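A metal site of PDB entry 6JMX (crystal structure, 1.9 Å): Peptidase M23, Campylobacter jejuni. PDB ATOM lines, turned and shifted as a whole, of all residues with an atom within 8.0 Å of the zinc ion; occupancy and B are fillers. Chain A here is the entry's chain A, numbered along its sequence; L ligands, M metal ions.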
ATOM      1  N   THR A 132      22.050  27.459 -10.307  1.00  0.00           N
ATOM      2  CA  THR A 132      22.549  27.004  -9.027  1.00  0.00           C
ATOM      3  C   THR A 132      23.572  25.893  -9.132  1.00  0.00           C
ATOM      4  O   THR A 132      24.313  25.666  -8.181  1.00  0.00           O
ATOM      5  CB  THR A 132      21.390  26.526  -8.137  1.00  0.00           C
ATOM      6  OG1 THR A 132      20.647  25.509  -8.834  1.00  0.00           O
ATOM      7  CG2 THR A 132      20.469  27.696  -7.842  1.00  0.00           C
ATOM      8  N   SER A 133      23.644  25.215 -10.273  1.00  0.00           N
ATOM      9  CA  SER A 133      24.653  24.178 -10.483  1.00  0.00           C
ATOM     10  C   SER A 133      24.960  24.097 -11.963  1.00  0.00           C
ATOM     11  O   SER A 133      24.111  23.657 -12.738  1.00  0.00           O
ATOM     12  CB  SER A 133      24.187  22.832  -9.931  1.00  0.00           C
ATOM     13  OG  SER A 133      25.241  21.895 -10.011  1.00  0.00           O
ATOM     14  N   ASP A 134      26.173  24.510 -12.337  1.00  0.00           N
ATOM     15  CA  ASP A 134      26.583  24.592 -13.728  1.00  0.00           C
ATOM     16  C   ASP A 134      26.667  23.224 -14.392  1.00  0.00           C
ATOM     17  O   ASP A 134      26.948  22.210 -13.749  1.00  0.00           O
ATOM     18  CB  ASP A 134      27.963  25.266 -13.838  1.00  0.00           C
ATOM     19  CG  ASP A 134      27.888  26.769 -13.841  1.00  0.00           C
ATOM     20  OD1 ASP A 134      27.241  27.331 -14.764  1.00  0.00           O
ATOM     21  OD2 ASP A 134      28.475  27.375 -12.933  1.00  0.00           O
ATOM     22  N   PHE A 135      26.475  23.211 -15.710  1.00  0.00           N
ATOM     23  CA  PHE A 135      26.739  22.021 -16.501  1.00  0.00           C
ATOM     24  C   PHE A 135      28.212  21.638 -16.397  1.00  0.00           C
ATOM     25  O   PHE A 135      29.092  22.505 -16.378  1.00  0.00           O
ATOM     26  CB  PHE A 135      26.372  22.268 -17.973  1.00  0.00           C
ATOM     27  CG  PHE A 135      26.800  21.175 -18.914  1.00  0.00           C
ATOM     28  CD1 PHE A 135      28.044  21.205 -19.533  1.00  0.00           C
ATOM     29  CD2 PHE A 135      25.943  20.128 -19.207  1.00  0.00           C
ATOM     30  CE1 PHE A 135      28.438  20.209 -20.401  1.00  0.00           C
ATOM     31  CE2 PHE A 135      26.325  19.122 -20.091  1.00  0.00           C
ATOM     32  CZ  PHE A 135      27.577  19.156 -20.681  1.00  0.00           C
ATOM     33  N   TYR A 148      29.530  13.469 -14.048  1.00  0.00           N
ATOM     34  CA  TYR A 148      29.483  14.904 -14.284  1.00  0.00           C
ATOM     35  C   TYR A 148      28.032  15.332 -14.375  1.00  0.00           C
ATOM     36  O   TYR A 148      27.132  14.520 -14.641  1.00  0.00           O
ATOM     37  CB  TYR A 148      30.261  15.291 -15.544  1.00  0.00           C
ATOM     38  CG  TYR A 148      29.529  14.956 -16.822  1.00  0.00           C
ATOM     39  CD1 TYR A 148      29.485  13.660 -17.304  1.00  0.00           C
ATOM     40  CD2 TYR A 148      28.867  15.947 -17.545  1.00  0.00           C
ATOM     41  CE1 TYR A 148      28.806  13.345 -18.475  1.00  0.00           C
ATOM     42  CE2 TYR A 148      28.184  15.640 -18.704  1.00  0.00           C
ATOM     43  CZ  TYR A 148      28.161  14.340 -19.158  1.00  0.00           C
ATOM     44  OH  TYR A 148      27.474  14.039 -20.324  1.00  0.00           O
ATOM     45  N   HIS A 149      27.802  16.617 -14.149  1.00  0.00           N
ATOM     46  CA  HIS A 149      26.462  17.176 -14.206  1.00  0.00           C
ATOM     47  C   HIS A 149      26.076  17.351 -15.672  1.00  0.00           C
ATOM     48  O   HIS A 149      26.639  18.201 -16.362  1.00  0.00           O
ATOM     49  CB  HIS A 149      26.426  18.504 -13.459  1.00  0.00           C
ATOM     50  CG  HIS A 149      25.050  19.053 -13.277  1.00  0.00           C
ATOM     51  ND1 HIS A 149      24.798  20.400 -13.149  1.00  0.00           N
ATOM     52  CD2 HIS A 149      23.859  18.425 -13.180  1.00  0.00           C
ATOM     53  CE1 HIS A 149      23.501  20.581 -12.995  1.00  0.00           C
ATOM     54  NE2 HIS A 149      22.906  19.398 -13.012  1.00  0.00           N
ATOM     55  N   SER A 150      25.096  16.587 -16.151  1.00  0.00           N
ATOM     56  CA  SER A 150      24.829  16.545 -17.587  1.00  0.00           C
ATOM     57  C   SER A 150      23.763  17.549 -18.035  1.00  0.00           C
ATOM     58  O   SER A 150      23.265  17.427 -19.160  1.00  0.00           O
ATOM     59  CB  SER A 150      24.402  15.132 -17.986  1.00  0.00           C
ATOM     60  OG  SER A 150      23.185  14.806 -17.347  1.00  0.00           O
ATOM     61  N   GLY A 151      23.408  18.497 -17.181  1.00  0.00           N
ATOM     62  CA  GLY A 151      22.589  19.622 -17.560  1.00  0.00           C
ATOM     63  C   GLY A 151      22.894  20.774 -16.633  1.00  0.00           C
ATOM     64  O   GLY A 151      23.928  20.769 -15.960  1.00  0.00           O
ATOM     65  N   THR A 152      21.994  21.732 -16.580  1.00  0.00           N
ATOM     66  CA  THR A 152      22.181  22.912 -15.746  1.00  0.00           C
ATOM     67  C   THR A 152      20.975  23.072 -14.837  1.00  0.00           C
ATOM     68  O   THR A 152      19.831  22.933 -15.288  1.00  0.00           O
ATOM     69  CB  THR A 152      22.360  24.171 -16.607  1.00  0.00           C
ATOM     70  OG1 THR A 152      23.430  23.958 -17.533  1.00  0.00           O
ATOM     71  CG2 THR A 152      22.758  25.331 -15.739  1.00  0.00           C
ATOM     72  N   ASP A 153      21.235  23.377 -13.563  1.00  0.00           N
ATOM     73  CA  ASP A 153      20.166  23.532 -12.568  1.00  0.00           C
ATOM     74  C   ASP A 153      19.839  25.001 -12.374  1.00  0.00           C
ATOM     75  O   ASP A 153      20.743  25.830 -12.237  1.00  0.00           O
ATOM     76  CB  ASP A 153      20.561  22.920 -11.226  1.00  0.00           C
ATOM     77  CG  ASP A 153      20.733  21.417 -11.293  1.00  0.00           C
ATOM     78  OD1 ASP A 153      20.223  20.804 -12.248  1.00  0.00           O
ATOM     79  OD2 ASP A 153      21.352  20.846 -10.374  1.00  0.00           O
ATOM     80  N   PHE A 154      18.543  25.319 -12.370  1.00  0.00           N
ATOM     81  CA  PHE A 154      18.037  26.655 -12.099  1.00  0.00           C
ATOM     82  C   PHE A 154      17.358  26.681 -10.738  1.00  0.00           C
ATOM     83  O   PHE A 154      16.678  25.717 -10.379  1.00  0.00           O
ATOM     84  CB  PHE A 154      17.000  27.076 -13.133  1.00  0.00           C
ATOM     85  CG  PHE A 154      17.575  27.414 -14.485  1.00  0.00           C
ATOM     86  CD1 PHE A 154      17.866  26.414 -15.392  1.00  0.00           C
ATOM     87  CD2 PHE A 154      17.755  28.723 -14.851  1.00  0.00           C
ATOM     88  CE1 PHE A 154      18.372  26.714 -16.635  1.00  0.00           C
ATOM     89  CE2 PHE A 154      18.259  29.051 -16.097  1.00  0.00           C
ATOM     90  CZ  PHE A 154      18.567  28.039 -16.997  1.00  0.00           C
ATOM     91  N   TYR A 196      13.631  18.188 -15.846  1.00  0.00           N
ATOM     92  CA  TYR A 196      13.637  17.068 -14.919  1.00  0.00           C
ATOM     93  C   TYR A 196      13.281  17.524 -13.506  1.00  0.00           C
ATOM     94  O   TYR A 196      13.403  18.700 -13.153  1.00  0.00           O
ATOM     95  CB  TYR A 196      15.016  16.396 -14.875  1.00  0.00           C
ATOM     96  CG  TYR A 196      15.400  15.669 -16.149  1.00  0.00           C
ATOM     97  CD1 TYR A 196      14.462  15.417 -17.148  1.00  0.00           C
ATOM     98  CD2 TYR A 196      16.709  15.271 -16.354  1.00  0.00           C
ATOM     99  CE1 TYR A 196      14.828  14.742 -18.310  1.00  0.00           C
ATOM    100  CE2 TYR A 196      17.091  14.611 -17.512  1.00  0.00           C
ATOM    101  CZ  TYR A 196      16.146  14.346 -18.487  1.00  0.00           C
ATOM    102  OH  TYR A 196      16.519  13.686 -19.639  1.00  0.00           O
ATOM    103  N   HIS A 197      12.864  16.530 -12.701  1.00  0.00           N
ATOM    104  CA  HIS A 197      12.543  16.677 -11.273  1.00  0.00           C
ATOM    105  C   HIS A 197      11.281  17.508 -11.037  1.00  0.00           C
ATOM    106  O   HIS A 197      11.122  18.116  -9.981  1.00  0.00           O
ATOM    107  CB  HIS A 197      13.734  17.266 -10.503  1.00  0.00           C
ATOM    108  CG  HIS A 197      15.013  16.546 -10.785  1.00  0.00           C
ATOM    109  ND1 HIS A 197      15.185  15.205 -10.547  1.00  0.00           N
ATOM    110  CD2 HIS A 197      16.185  16.978 -11.317  1.00  0.00           C
ATOM    111  CE1 HIS A 197      16.404  14.837 -10.911  1.00  0.00           C
ATOM    112  NE2 HIS A 197      17.031  15.895 -11.376  1.00  0.00           N
ATOM    113  N   ARG A 223      15.991  11.755  -8.109  1.00  0.00           N
ATOM    114  CA  ARG A 223      17.229  11.914  -7.342  1.00  0.00           C
ATOM    115  C   ARG A 223      17.622  13.390  -7.331  1.00  0.00           C
ATOM    116  O   ARG A 223      18.056  13.925  -8.351  1.00  0.00           O
ATOM    117  CB  ARG A 223      18.336  11.050  -7.928  1.00  0.00           C
ATOM    118  CG  ARG A 223      19.710  11.234  -7.281  1.00  0.00           C
ATOM    119  CD  ARG A 223      20.772  10.399  -7.996  1.00  0.00           C
ATOM    120  NE  ARG A 223      20.744  10.599  -9.445  1.00  0.00           N
ATOM    121  CZ  ARG A 223      21.499   9.916 -10.309  1.00  0.00           C
ATOM    122  NH1 ARG A 223      22.344   8.989  -9.878  1.00  0.00           N
ATOM    123  NH2 ARG A 223      21.393  10.173 -11.612  1.00  0.00           N
ATOM    124  N   VAL A 224      17.470  14.049  -6.182  1.00  0.00           N
ATOM    125  CA  VAL A 224      17.712  15.484  -6.055  1.00  0.00           C
ATOM    126  C   VAL A 224      18.272  15.795  -4.675  1.00  0.00           C
ATOM    127  O   VAL A 224      17.979  15.094  -3.700  1.00  0.00           O
ATOM    128  CB  VAL A 224      16.438  16.325  -6.260  1.00  0.00           C
ATOM    129  CG1 VAL A 224      16.004  16.294  -7.690  1.00  0.00           C
ATOM    130  CG2 VAL A 224      15.333  15.846  -5.331  1.00  0.00           C
ATOM    131  N   HIS A 228      14.551  22.279  -7.417  1.00  0.00           N
ATOM    132  CA  HIS A 228      15.211  23.046  -8.483  1.00  0.00           C
ATOM    133  C   HIS A 228      14.665  22.526  -9.810  1.00  0.00           C
ATOM    134  O   HIS A 228      13.952  21.518  -9.853  1.00  0.00           O
ATOM    135  CB  HIS A 228      16.733  22.916  -8.447  1.00  0.00           C
ATOM    136  CG  HIS A 228      17.225  21.533  -8.755  1.00  0.00           C
ATOM    137  ND1 HIS A 228      17.237  20.520  -7.820  1.00  0.00           N
ATOM    138  CD2 HIS A 228      17.735  20.990  -9.889  1.00  0.00           C
ATOM    139  CE1 HIS A 228      17.717  19.414  -8.365  1.00  0.00           C
ATOM    140  NE2 HIS A 228      18.028  19.673  -9.620  1.00  0.00           N
ATOM    141  N   LEU A 229      14.984  23.240 -10.902  1.00  0.00           N
ATOM    142  CA  LEU A 229      14.743  22.731 -12.252  1.00  0.00           C
ATOM    143  C   LEU A 229      16.074  22.286 -12.836  1.00  0.00           C
ATOM    144  O   LEU A 229      17.047  23.041 -12.791  1.00  0.00           O
ATOM    145  CB  LEU A 229      14.131  23.792 -13.179  1.00  0.00           C
ATOM    146  CG  LEU A 229      14.130  23.297 -14.625  1.00  0.00           C
ATOM    147  CD1 LEU A 229      13.013  22.289 -14.866  1.00  0.00           C
ATOM    148  CD2 LEU A 229      14.063  24.449 -15.635  1.00  0.00           C
ATOM    149  N   HIS A 230      16.123  21.063 -13.361  1.00  0.00           N
ATOM    150  CA  HIS A 230      17.275  20.612 -14.140  1.00  0.00           C
ATOM    151  C   HIS A 230      16.913  20.709 -15.622  1.00  0.00           C
ATOM    152  O   HIS A 230      15.945  20.098 -16.068  1.00  0.00           O
ATOM    153  CB  HIS A 230      17.671  19.176 -13.763  1.00  0.00           C
ATOM    154  CG  HIS A 230      18.660  18.545 -14.698  1.00  0.00           C
ATOM    155  ND1 HIS A 230      19.988  18.393 -14.369  1.00  0.00           N
ATOM    156  CD2 HIS A 230      18.514  18.057 -15.952  1.00  0.00           C
ATOM    157  CE1 HIS A 230      20.616  17.812 -15.374  1.00  0.00           C
ATOM    158  NE2 HIS A 230      19.754  17.601 -16.355  1.00  0.00           N
ATOM    159  N   PHE A 231      17.701  21.482 -16.377  1.00  0.00           N
ATOM    160  CA  PHE A 231      17.475  21.715 -17.792  1.00  0.00           C
ATOM    161  C   PHE A 231      18.613  21.092 -18.573  1.00  0.00           C
ATOM    162  O   PHE A 231      19.785  21.342 -18.254  1.00  0.00           O
ATOM    163  CB  PHE A 231      17.367  23.212 -18.079  1.00  0.00           C
ATOM    164  CG  PHE A 231      17.154  23.562 -19.544  1.00  0.00           C
ATOM    165  CD1 PHE A 231      15.987  23.205 -20.196  1.00  0.00           C
ATOM    166  CD2 PHE A 231      18.114  24.271 -20.249  1.00  0.00           C
ATOM    167  CE1 PHE A 231      15.777  23.537 -21.538  1.00  0.00           C
ATOM    168  CE2 PHE A 231      17.915  24.611 -21.592  1.00  0.00           C
ATOM    169  CZ  PHE A 231      16.734  24.226 -22.229  1.00  0.00           C
ATOM    170  N   GLY A 232      18.296  20.307 -19.602  1.00  0.00           N
ATOM    171  CA  GLY A 232      19.331  19.697 -20.406  1.00  0.00           C
ATOM    172  C   GLY A 232      19.026  19.797 -21.895  1.00  0.00           C
ATOM    173  O   GLY A 232      17.886  20.003 -22.306  1.00  0.00           O
HETATM  174  O1  LIG L   1      21.371  18.872  -8.068  1.00  0.00           O
HETATM  175  O2  LIG L   1      20.036  17.598  -6.875  1.00  0.00           O
HETATM  176  C1  LIG L   1      20.730  17.816  -7.893  1.00  0.00           C
HETATM  177  C2  LIG L   1      20.806  16.753  -8.960  1.00  0.00           C
HETATM  178  O3  LIG L   1      19.652  15.913  -8.879  1.00  0.00           O
HETATM  179  C3  LIG L   1      20.858  17.419 -10.335  1.00  0.00           C
HETATM  180  O4  LIG L   1      19.544  17.868 -10.696  1.00  0.00           O
HETATM  181  C4  LIG L   1      21.339  16.429 -11.354  1.00  0.00           C
HETATM  182  O5  LIG L   1      21.589  16.842 -12.506  1.00  0.00           O
HETATM  183  O6  LIG L   1      21.491  15.231 -11.007  1.00  0.00           O
HETATM  184 ZN    ZN M   1      20.967  18.907 -12.599  1.00  0.00          ZN
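The backbone carbonyl oxygen of Ser 133 sits at hydrogen-bond distance from the backbone NH of Asp 153 (3.0 Å). O of Asp 153 is in hydrogen-bond range of N of Thr 132, at 2.8 Å. ND1 of His 149 sits close to O of Ser 133. A ring nitrogen (ND1) of His 149 is in hydrogen-bond range of the backbone carbonyl oxygen of Gly 151 (3.0 Å). A ring nitrogen (ND1) of His 149 is in hydrogen-bond range of the backbone carbonyl oxygen of Asp 134. The backbone NH (N) of Tyr 196 sits at hydrogen-bond distance from the backbone carbonyl oxygen (O) of His 230, at 3.0 Å.
The zinc ion is bound by a ring nitrogen (NE2) of His 149. The zinc ion is bound by OD1 of Asp 153, at 2.1 Å. ND1 of His 230 binds the zinc ion (2.1 Å). O5 of the ligand is bound to the zinc ion, at 2.2 Å. O4 of the ligand binds the zinc ion.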
